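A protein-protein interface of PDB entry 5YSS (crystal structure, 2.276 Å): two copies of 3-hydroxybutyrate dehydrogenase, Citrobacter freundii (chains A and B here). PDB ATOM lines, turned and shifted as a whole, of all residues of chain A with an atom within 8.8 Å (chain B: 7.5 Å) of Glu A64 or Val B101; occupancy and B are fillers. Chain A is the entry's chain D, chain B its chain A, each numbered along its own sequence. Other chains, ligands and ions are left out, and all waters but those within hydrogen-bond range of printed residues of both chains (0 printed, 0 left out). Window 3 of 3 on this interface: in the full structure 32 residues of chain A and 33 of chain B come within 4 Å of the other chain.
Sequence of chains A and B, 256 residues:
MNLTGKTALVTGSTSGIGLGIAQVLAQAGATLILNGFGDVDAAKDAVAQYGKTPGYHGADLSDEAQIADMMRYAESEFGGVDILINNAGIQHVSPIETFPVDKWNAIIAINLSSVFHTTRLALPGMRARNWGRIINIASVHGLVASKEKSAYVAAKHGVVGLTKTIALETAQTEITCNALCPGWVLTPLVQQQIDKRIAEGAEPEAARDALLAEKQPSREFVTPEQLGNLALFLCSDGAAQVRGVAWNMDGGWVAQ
Of the 22 printed residues of chain A, 4 touch a printed residue of chain B. Hydrophobic or aromatic side chains of chain A within 4 Å of the printed part of chain B: Ile A108 and Phe A116. Hydrophobic or aromatic side chains of chain B that line the printed part of chain A: Val B101, Trp B104 and Ile B108.
Of the printed residues of chain B, Glu A64 touches Val B101 (3.3 Å) and Asn B105 (3.4 Å). Val B101 touches just one residue of chain A: Glu A64. Printed residues of chain A within 4 Å of Asn B105: Glu A64. Of the printed residues of chain A, Ile B108 touches Ile A108. Ile A67 touches none of the printed residues of chain B. The nearest printed residue of chain B that does not touch Ser A113 is Ile B108 (4.8 Å).
OE2 of Glu A64 lies close to OD1 of Asn B105 (3.4 Å). The indole nitrogen of Trp B104 lies within hydrogen-bond range of the side-chain hydroxyl of Ser A113 (2.8 Å).
Among the printed residues, pairs that only touch across the chains: Glu A64 with Val B101 (3.3 Å), Phe A116 with Trp B104 (3.5 Å), Phe A116 with Phe B99 (3.7 Å) and Ile A108 with Ile B108 (3.97 Å).
A ring nitrogen (NE2) of His A117 lies within hydrogen-bond range of the side-chain carboxylate (OE2) of Glu A64 (3.1 Å). The backbone carbonyl oxygen (O) of Ile A108 sits at hydrogen-bond distance from the backbone NH (N) of Ser A113, 2.9 Å away.
Ile B108 touches its own counterpart, Ile A108. Position printed for both chains: 108. Of the 6 pairs that touch across the chains among the printed residues, 1 has its exchanged pair printed and touching as well.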
ATOM      1  N   ALA A  59      29.627 -17.891   7.417  1.00  0.00           N
ATOM      2  CA  ALA A  59      29.176 -18.991   8.259  1.00  0.00           C
ATOM      3  C   ALA A  59      29.876 -20.289   7.878  1.00  0.00           C
ATOM      4  O   ALA A  59      29.873 -20.690   6.716  1.00  0.00           O
ATOM      5  CB  ALA A  59      27.668 -19.155   8.169  1.00  0.00           C
ATOM      6  N   ASP A  60      30.512 -20.905   8.865  1.00  0.00           N
ATOM      7  CA  ASP A  60      30.966 -22.280   8.754  1.00  0.00           C
ATOM      8  C   ASP A  60      29.735 -23.196   8.802  1.00  0.00           C
ATOM      9  O   ASP A  60      29.107 -23.366   9.854  1.00  0.00           O
ATOM     10  CB  ASP A  60      31.947 -22.611   9.879  1.00  0.00           C
ATOM     11  CG  ASP A  60      32.211 -24.093  10.005  1.00  0.00           C
ATOM     12  OD1 ASP A  60      31.981 -24.831   9.024  1.00  0.00           O
ATOM     13  OD2 ASP A  60      32.655 -24.528  11.091  1.00  0.00           O
ATOM     14  N   LEU A  61      29.403 -23.790   7.661  1.00  0.00           N
ATOM     15  CA  LEU A  61      28.173 -24.564   7.526  1.00  0.00           C
ATOM     16  C   LEU A  61      28.118 -25.832   8.378  1.00  0.00           C
ATOM     17  O   LEU A  61      27.044 -26.397   8.561  1.00  0.00           O
ATOM     18  CB  LEU A  61      27.953 -24.925   6.061  1.00  0.00           C
ATOM     19  CG  LEU A  61      27.531 -23.676   5.293  1.00  0.00           C
ATOM     20  CD1 LEU A  61      27.855 -23.823   3.823  1.00  0.00           C
ATOM     21  CD2 LEU A  61      26.050 -23.409   5.500  1.00  0.00           C
ATOM     22  N   SER A  62      29.261 -26.267   8.907  1.00  0.00           N
ATOM     23  CA  SER A  62      29.290 -27.436   9.785  1.00  0.00           C
ATOM     24  C   SER A  62      28.754 -27.099  11.175  1.00  0.00           C
ATOM     25  O   SER A  62      28.664 -27.966  12.043  1.00  0.00           O
ATOM     26  CB  SER A  62      30.712 -27.997   9.890  1.00  0.00           C
ATOM     27  OG  SER A  62      31.622 -27.034  10.395  1.00  0.00           O
ATOM     28  N   ASP A  63      28.387 -25.835  11.376  1.00  0.00           N
ATOM     29  CA  ASP A  63      27.952 -25.356  12.682  1.00  0.00           C
ATOM     30  C   ASP A  63      26.563 -24.743  12.585  1.00  0.00           C
ATOM     31  O   ASP A  63      26.356 -23.729  11.910  1.00  0.00           O
ATOM     32  CB  ASP A  63      28.954 -24.340  13.234  1.00  0.00           C
ATOM     33  CG  ASP A  63      28.614 -23.873  14.641  1.00  0.00           C
ATOM     34  OD1 ASP A  63      27.672 -24.418  15.259  1.00  0.00           O
ATOM     35  OD2 ASP A  63      29.311 -22.961  15.137  1.00  0.00           O
ATOM     36  N   GLU A  64      25.617 -25.374  13.275  1.00  0.00           N
ATOM     37  CA  GLU A  64      24.217 -24.992  13.217  1.00  0.00           C
ATOM     38  C   GLU A  64      24.039 -23.546  13.694  1.00  0.00           C
ATOM     39  O   GLU A  64      23.245 -22.791  13.127  1.00  0.00           O
ATOM     40  CB  GLU A  64      23.383 -25.986  14.045  1.00  0.00           C
ATOM     41  CG  GLU A  64      23.933 -27.425  13.930  1.00  0.00           C
ATOM     42  CD  GLU A  64      23.043 -28.506  14.565  1.00  0.00           C
ATOM     43  OE1 GLU A  64      22.544 -28.297  15.693  1.00  0.00           O
ATOM     44  OE2 GLU A  64      22.854 -29.576  13.932  1.00  0.00           O
ATOM     45  N   ALA A  65      24.814 -23.154  14.704  1.00  0.00           N
ATOM     46  CA  ALA A  65      24.728 -21.805  15.262  1.00  0.00           C
ATOM     47  C   ALA A  65      25.097 -20.728  14.240  1.00  0.00           C
ATOM     48  O   ALA A  65      24.420 -19.712  14.138  1.00  0.00           O
ATOM     49  CB  ALA A  65      25.618 -21.683  16.489  1.00  0.00           C
ATOM     50  N   GLN A  66      26.167 -20.951  13.483  1.00  0.00           N
ATOM     51  CA  GLN A  66      26.615 -19.955  12.513  1.00  0.00           C
ATOM     52  C   GLN A  66      25.636 -19.816  11.354  1.00  0.00           C
ATOM     53  O   GLN A  66      25.557 -18.765  10.731  1.00  0.00           O
ATOM     54  CB  GLN A  66      28.007 -20.301  11.984  1.00  0.00           C
ATOM     55  CG  GLN A  66      29.119 -20.202  13.027  1.00  0.00           C
ATOM     56  CD  GLN A  66      30.488 -20.544  12.457  1.00  0.00           C
ATOM     57  OE1 GLN A  66      30.918 -19.969  11.460  1.00  0.00           O
ATOM     58  NE2 GLN A  66      31.172 -21.494  13.082  1.00  0.00           N
ATOM     59  N   ILE A  67      24.881 -20.869  11.066  1.00  0.00           N
ATOM     60  CA  ILE A  67      23.907 -20.802   9.984  1.00  0.00           C
ATOM     61  C   ILE A  67      22.731 -19.931  10.391  1.00  0.00           C
ATOM     62  O   ILE A  67      22.270 -19.092   9.616  1.00  0.00           O
ATOM     63  CB  ILE A  67      23.394 -22.190   9.583  1.00  0.00           C
ATOM     64  CG1 ILE A  67      24.562 -23.097   9.204  1.00  0.00           C
ATOM     65  CG2 ILE A  67      22.416 -22.075   8.414  1.00  0.00           C
ATOM     66  CD1 ILE A  67      24.163 -24.548   8.998  1.00  0.00           C
ATOM     67  N   ALA A  68      22.245 -20.139  11.612  1.00  0.00           N
ATOM     68  CA  ALA A  68      21.181 -19.310  12.164  1.00  0.00           C
ATOM     69  C   ALA A  68      21.582 -17.832  12.131  1.00  0.00           C
ATOM     70  O   ALA A  68      20.818 -16.988  11.671  1.00  0.00           O
ATOM     71  CB  ALA A  68      20.850 -19.740  13.574  1.00  0.00           C
ATOM     72  N   ASP A  69      22.787 -17.533  12.607  1.00  0.00           N
ATOM     73  CA  ASP A  69      23.324 -16.175  12.552  1.00  0.00           C
ATOM     74  C   ASP A  69      23.269 -15.623  11.133  1.00  0.00           C
ATOM     75  O   ASP A  69      22.746 -14.529  10.895  1.00  0.00           O
ATOM     76  CB  ASP A  69      24.765 -16.146  13.075  1.00  0.00           C
ATOM     77  CG  ASP A  69      24.834 -15.916  14.577  1.00  0.00           C
ATOM     78  OD1 ASP A  69      23.764 -15.839  15.230  1.00  0.00           O
ATOM     79  OD2 ASP A  69      25.960 -15.817  15.107  1.00  0.00           O
ATOM     80  N   MET A  70      23.792 -16.410  10.198  1.00  0.00           N
ATOM     81  CA  MET A  70      23.807 -16.063   8.784  1.00  0.00           C
ATOM     82  C   MET A  70      22.421 -15.788   8.201  1.00  0.00           C
ATOM     83  O   MET A  70      22.259 -14.874   7.393  1.00  0.00           O
ATOM     84  CB  MET A  70      24.483 -17.179   7.987  1.00  0.00           C
ATOM     85  CG  MET A  70      24.411 -17.009   6.487  1.00  0.00           C
ATOM     86  SD  MET A  70      25.065 -18.464   5.658  1.00  0.00           S
ATOM     87  CE  MET A  70      25.144 -17.873   3.993  1.00  0.00           C
ATOM     88  N   MET A  71      21.421 -16.570   8.596  1.00  0.00           N
ATOM     89  CA  MET A  71      20.091 -16.373   8.030  1.00  0.00           C
ATOM     90  C   MET A  71      19.467 -15.082   8.552  1.00  0.00           C
ATOM     91  O   MET A  71      18.848 -14.344   7.788  1.00  0.00           O
ATOM     92  CB  MET A  71      19.181 -17.570   8.317  1.00  0.00           C
ATOM     93  CG  MET A  71      19.662 -18.872   7.669  1.00  0.00           C
ATOM     94  SD  MET A  71      20.010 -18.730   5.894  1.00  0.00           S
ATOM     95  CE  MET A  71      18.360 -18.663   5.213  1.00  0.00           C
ATOM     96  N   ILE A 108      28.594 -35.128   6.372  1.00  0.00           N
ATOM     97  CA  ILE A 108      27.162 -35.117   6.667  1.00  0.00           C
ATOM     98  C   ILE A 108      26.696 -33.715   7.075  1.00  0.00           C
ATOM     99  O   ILE A 108      25.706 -33.198   6.549  1.00  0.00           O
ATOM    100  CB  ILE A 108      26.781 -36.103   7.798  1.00  0.00           C
ATOM    101  CG1 ILE A 108      27.129 -37.551   7.427  1.00  0.00           C
ATOM    102  CG2 ILE A 108      25.299 -35.980   8.121  1.00  0.00           C
ATOM    103  CD1 ILE A 108      26.447 -38.066   6.175  1.00  0.00           C
ATOM    104  N   ALA A 109      27.416 -33.107   8.013  1.00  0.00           N
ATOM    105  CA  ALA A 109      27.037 -31.805   8.540  1.00  0.00           C
ATOM    106  C   ALA A 109      26.929 -30.769   7.420  1.00  0.00           C
ATOM    107  O   ALA A 109      25.932 -30.070   7.304  1.00  0.00           O
ATOM    108  CB  ALA A 109      28.032 -31.348   9.592  1.00  0.00           C
ATOM    109  N   SER A 113      23.196 -31.753   6.290  1.00  0.00           N
ATOM    110  CA  SER A 113      22.461 -31.058   7.346  1.00  0.00           C
ATOM    111  C   SER A 113      22.336 -29.539   7.145  1.00  0.00           C
ATOM    112  O   SER A 113      21.381 -28.926   7.617  1.00  0.00           O
ATOM    113  CB  SER A 113      23.106 -31.351   8.699  1.00  0.00           C
ATOM    114  OG  SER A 113      22.778 -32.659   9.119  1.00  0.00           O
ATOM    115  N   SER A 114      23.299 -28.934   6.457  1.00  0.00           N
ATOM    116  CA  SER A 114      23.254 -27.499   6.199  1.00  0.00           C
ATOM    117  C   SER A 114      22.060 -27.135   5.316  1.00  0.00           C
ATOM    118  O   SER A 114      21.483 -26.053   5.454  1.00  0.00           O
ATOM    119  CB  SER A 114      24.561 -27.022   5.552  1.00  0.00           C
ATOM    120  OG  SER A 114      24.687 -27.531   4.236  1.00  0.00           O
ATOM    121  N   PHE A 116      19.197 -28.732   5.373  1.00  0.00           N
ATOM    122  CA  PHE A 116      18.084 -28.747   6.307  1.00  0.00           C
ATOM    123  C   PHE A 116      18.004 -27.416   7.049  1.00  0.00           C
ATOM    124  O   PHE A 116      16.940 -26.830   7.163  1.00  0.00           O
ATOM    125  CB  PHE A 116      18.225 -29.905   7.302  1.00  0.00           C
ATOM    126  CG  PHE A 116      17.287 -29.820   8.475  1.00  0.00           C
ATOM    127  CD1 PHE A 116      15.935 -30.070   8.318  1.00  0.00           C
ATOM    128  CD2 PHE A 116      17.761 -29.498   9.739  1.00  0.00           C
ATOM    129  CE1 PHE A 116      15.058 -29.998   9.403  1.00  0.00           C
ATOM    130  CE2 PHE A 116      16.896 -29.417  10.828  1.00  0.00           C
ATOM    131  CZ  PHE A 116      15.538 -29.675  10.657  1.00  0.00           C
ATOM    132  N   HIS A 117      19.141 -26.940   7.539  1.00  0.00           N
ATOM    133  CA  HIS A 117      19.162 -25.746   8.369  1.00  0.00           C
ATOM    134  C   HIS A 117      18.834 -24.465   7.597  1.00  0.00           C
ATOM    135  O   HIS A 117      18.057 -23.651   8.084  1.00  0.00           O
ATOM    136  CB  HIS A 117      20.520 -25.604   9.056  1.00  0.00           C
ATOM    137  CG  HIS A 117      20.765 -26.622  10.123  1.00  0.00           C
ATOM    138  ND1 HIS A 117      19.876 -26.845  11.155  1.00  0.00           N
ATOM    139  CD2 HIS A 117      21.794 -27.475  10.323  1.00  0.00           C
ATOM    140  CE1 HIS A 117      20.347 -27.791  11.942  1.00  0.00           C
ATOM    141  NE2 HIS A 117      21.510 -28.194  11.462  1.00  0.00           N
ATOM    142  N   THR A 118      19.409 -24.277   6.409  1.00  0.00           N
ATOM    143  CA  THR A 118      19.060 -23.096   5.619  1.00  0.00           C
ATOM    144  C   THR A 118      17.593 -23.136   5.199  1.00  0.00           C
ATOM    145  O   THR A 118      16.866 -22.160   5.392  1.00  0.00           O
ATOM    146  CB  THR A 118      19.942 -22.931   4.353  1.00  0.00           C
ATOM    147  OG1 THR A 118      19.784 -24.056   3.475  1.00  0.00           O
ATOM    148  CG2 THR A 118      21.394 -22.761   4.737  1.00  0.00           C
ATOM    149  N   ARG A 120      15.116 -24.769   6.471  1.00  0.00           N
ATOM    150  CA  ARG A 120      14.388 -24.532   7.718  1.00  0.00           C
ATOM    151  C   ARG A 120      14.099 -23.048   7.975  1.00  0.00           C
ATOM    152  O   ARG A 120      12.963 -22.664   8.249  1.00  0.00           O
ATOM    153  CB  ARG A 120      15.190 -25.100   8.899  1.00  0.00           C
ATOM    154  CG  ARG A 120      14.403 -25.354  10.180  1.00  0.00           C
ATOM    155  CD  ARG A 120      15.239 -26.173  11.192  1.00  0.00           C
ATOM    156  NE  ARG A 120      15.756 -25.349  12.287  1.00  0.00           N
ATOM    157  CZ  ARG A 120      16.961 -24.780  12.297  1.00  0.00           C
ATOM    158  NH1 ARG A 120      17.782 -24.952  11.278  1.00  0.00           N
ATOM    159  NH2 ARG A 120      17.348 -24.041  13.330  1.00  0.00           N
ATOM    160  N   LEU A 121      15.138 -22.226   7.881  1.00  0.00           N
ATOM    161  CA  LEU A 121      15.082 -20.828   8.307  1.00  0.00           C
ATOM    162  C   LEU A 121      14.642 -19.825   7.231  1.00  0.00           C
ATOM    163  O   LEU A 121      14.304 -18.686   7.547  1.00  0.00           O
ATOM    164  CB  LEU A 121      16.457 -20.409   8.841  1.00  0.00           C
ATOM    165  CG  LEU A 121      16.955 -21.237  10.028  1.00  0.00           C
ATOM    166  CD1 LEU A 121      18.396 -20.917  10.333  1.00  0.00           C
ATOM    167  CD2 LEU A 121      16.063 -21.008  11.252  1.00  0.00           C
ATOM    168  N   THR B  98       9.080 -26.333  11.493  1.00  0.00           N
ATOM    169  CA  THR B  98       8.999 -26.540  12.932  1.00  0.00           C
ATOM    170  C   THR B  98       9.568 -27.910  13.331  1.00  0.00           C
ATOM    171  O   THR B  98       9.136 -28.515  14.318  1.00  0.00           O
ATOM    172  CB  THR B  98       7.537 -26.404  13.430  1.00  0.00           C
ATOM    173  OG1 THR B  98       6.694 -27.281  12.678  1.00  0.00           O
ATOM    174  CG2 THR B  98       7.038 -24.982  13.241  1.00  0.00           C
ATOM    175  N   PHE B  99      10.540 -28.391  12.560  1.00  0.00           N
ATOM    176  CA  PHE B  99      11.163 -29.688  12.813  1.00  0.00           C
ATOM    177  C   PHE B  99      12.313 -29.541  13.810  1.00  0.00           C
ATOM    178  O   PHE B  99      13.340 -28.964  13.485  1.00  0.00           O
ATOM    179  CB  PHE B  99      11.665 -30.300  11.502  1.00  0.00           C
ATOM    180  CG  PHE B  99      11.830 -31.798  11.543  1.00  0.00           C
ATOM    181  CD1 PHE B  99      12.866 -32.383  12.259  1.00  0.00           C
ATOM    182  CD2 PHE B  99      10.958 -32.619  10.845  1.00  0.00           C
ATOM    183  CE1 PHE B  99      13.020 -33.753  12.286  1.00  0.00           C
ATOM    184  CE2 PHE B  99      11.108 -33.993  10.867  1.00  0.00           C
ATOM    185  CZ  PHE B  99      12.145 -34.561  11.589  1.00  0.00           C
ATOM    186  N   PRO B 100      12.143 -30.078  15.031  1.00  0.00           N
ATOM    187  CA  PRO B 100      13.169 -29.936  16.071  1.00  0.00           C
ATOM    188  C   PRO B 100      14.558 -30.395  15.615  1.00  0.00           C
ATOM    189  O   PRO B 100      14.716 -31.446  14.966  1.00  0.00           O
ATOM    190  CB  PRO B 100      12.644 -30.823  17.205  1.00  0.00           C
ATOM    191  CG  PRO B 100      11.167 -30.862  16.989  1.00  0.00           C
ATOM    192  CD  PRO B 100      10.991 -30.864  15.499  1.00  0.00           C
ATOM    193  N   VAL B 101      15.557 -29.593  15.959  1.00  0.00           N
ATOM    194  CA  VAL B 101      16.937 -29.896  15.628  1.00  0.00           C
ATOM    195  C   VAL B 101      17.366 -31.238  16.233  1.00  0.00           C
ATOM    196  O   VAL B 101      17.915 -32.095  15.534  1.00  0.00           O
ATOM    197  CB  VAL B 101      17.866 -28.766  16.108  1.00  0.00           C
ATOM    198  CG1 VAL B 101      19.290 -29.017  15.668  1.00  0.00           C
ATOM    199  CG2 VAL B 101      17.378 -27.439  15.557  1.00  0.00           C
ATOM    200  N   ASP B 102      17.094 -31.424  17.522  1.00  0.00           N
ATOM    201  CA  ASP B 102      17.514 -32.623  18.237  1.00  0.00           C
ATOM    202  C   ASP B 102      16.938 -33.876  17.587  1.00  0.00           C
ATOM    203  O   ASP B 102      17.598 -34.922  17.550  1.00  0.00           O
ATOM    204  CB  ASP B 102      17.120 -32.545  19.723  1.00  0.00           C
ATOM    205  CG  ASP B 102      15.607 -32.486  19.943  1.00  0.00           C
ATOM    206  OD1 ASP B 102      15.010 -31.404  19.767  1.00  0.00           O
ATOM    207  OD2 ASP B 102      15.006 -33.519  20.325  1.00  0.00           O
ATOM    208  N   LYS B 103      15.727 -33.759  17.042  1.00  0.00           N
ATOM    209  CA  LYS B 103      15.101 -34.866  16.323  1.00  0.00           C
ATOM    210  C   LYS B 103      15.787 -35.131  14.986  1.00  0.00           C
ATOM    211  O   LYS B 103      15.994 -36.296  14.623  1.00  0.00           O
ATOM    212  CB  LYS B 103      13.618 -34.598  16.106  1.00  0.00           C
ATOM    213  CG  LYS B 103      12.779 -34.734  17.386  1.00  0.00           C
ATOM    214  CD  LYS B 103      12.950 -36.125  18.008  1.00  0.00           C
ATOM    215  CE  LYS B 103      11.980 -36.362  19.168  1.00  0.00           C
ATOM    216  NZ  LYS B 103      10.605 -36.517  18.660  1.00  0.00           N
ATOM    217  N   TRP B 104      16.148 -34.062  14.264  1.00  0.00           N
ATOM    218  CA  TRP B 104      16.931 -34.196  13.032  1.00  0.00           C
ATOM    219  C   TRP B 104      18.248 -34.931  13.292  1.00  0.00           C
ATOM    220  O   TRP B 104      18.584 -35.903  12.601  1.00  0.00           O
ATOM    221  CB  TRP B 104      17.222 -32.825  12.390  1.00  0.00           C
ATOM    222  CG  TRP B 104      18.247 -32.903  11.276  1.00  0.00           C
ATOM    223  CD1 TRP B 104      19.613 -32.797  11.400  1.00  0.00           C
ATOM    224  CD2 TRP B 104      17.993 -33.126   9.878  1.00  0.00           C
ATOM    225  NE1 TRP B 104      20.213 -32.939  10.173  1.00  0.00           N
ATOM    226  CE2 TRP B 104      19.246 -33.143   9.223  1.00  0.00           C
ATOM    227  CE3 TRP B 104      16.836 -33.306   9.120  1.00  0.00           C
ATOM    228  CZ2 TRP B 104      19.366 -33.337   7.851  1.00  0.00           C
ATOM    229  CZ3 TRP B 104      16.957 -33.500   7.760  1.00  0.00           C
ATOM    230  CH2 TRP B 104      18.217 -33.517   7.137  1.00  0.00           C
ATOM    231  N   ASN B 105      19.002 -34.468  14.286  1.00  0.00           N
ATOM    232  CA  ASN B 105      20.283 -35.099  14.599  1.00  0.00           C
ATOM    233  C   ASN B 105      20.111 -36.547  15.035  1.00  0.00           C
ATOM    234  O   ASN B 105      20.909 -37.410  14.682  1.00  0.00           O
ATOM    235  CB  ASN B 105      21.018 -34.306  15.682  1.00  0.00           C
ATOM    236  CG  ASN B 105      21.383 -32.894  15.226  1.00  0.00           C
ATOM    237  OD1 ASN B 105      21.289 -32.574  14.045  1.00  0.00           O
ATOM    238  ND2 ASN B 105      21.802 -32.051  16.160  1.00  0.00           N
ATOM    239  N   ALA B 106      19.052 -36.823  15.786  1.00  0.00           N
ATOM    240  CA  ALA B 106      18.829 -38.173  16.293  1.00  0.00           C
ATOM    241  C   ALA B 106      18.503 -39.134  15.156  1.00  0.00           C
ATOM    242  O   ALA B 106      19.039 -40.245  15.085  1.00  0.00           O
ATOM    243  CB  ALA B 106      17.721 -38.170  17.321  1.00  0.00           C
ATOM    244  N   ILE B 107      17.638 -38.688  14.255  1.00  0.00           N
ATOM    245  CA  ILE B 107      17.208 -39.502  13.128  1.00  0.00           C
ATOM    246  C   ILE B 107      18.363 -39.811  12.174  1.00  0.00           C
ATOM    247  O   ILE B 107      18.510 -40.944  11.724  1.00  0.00           O
ATOM    248  CB  ILE B 107      16.064 -38.810  12.370  1.00  0.00           C
ATOM    249  CG1 ILE B 107      14.800 -38.797  13.246  1.00  0.00           C
ATOM    250  CG2 ILE B 107      15.796 -39.512  11.053  1.00  0.00           C
ATOM    251  CD1 ILE B 107      13.580 -38.175  12.596  1.00  0.00           C
ATOM    252  N   ILE B 108      19.175 -38.795  11.867  1.00  0.00           N
ATOM    253  CA  ILE B 108      20.340 -38.969  11.016  1.00  0.00           C
ATOM    254  C   ILE B 108      21.336 -39.926  11.658  1.00  0.00           C
ATOM    255  O   ILE B 108      21.913 -40.787  10.988  1.00  0.00           O
ATOM    256  CB  ILE B 108      21.067 -37.613  10.723  1.00  0.00           C
ATOM    257  CG1 ILE B 108      20.126 -36.606  10.050  1.00  0.00           C
ATOM    258  CG2 ILE B 108      22.241 -37.844   9.843  1.00  0.00           C
ATOM    259  CD1 ILE B 108      19.642 -37.020   8.679  1.00  0.00           C
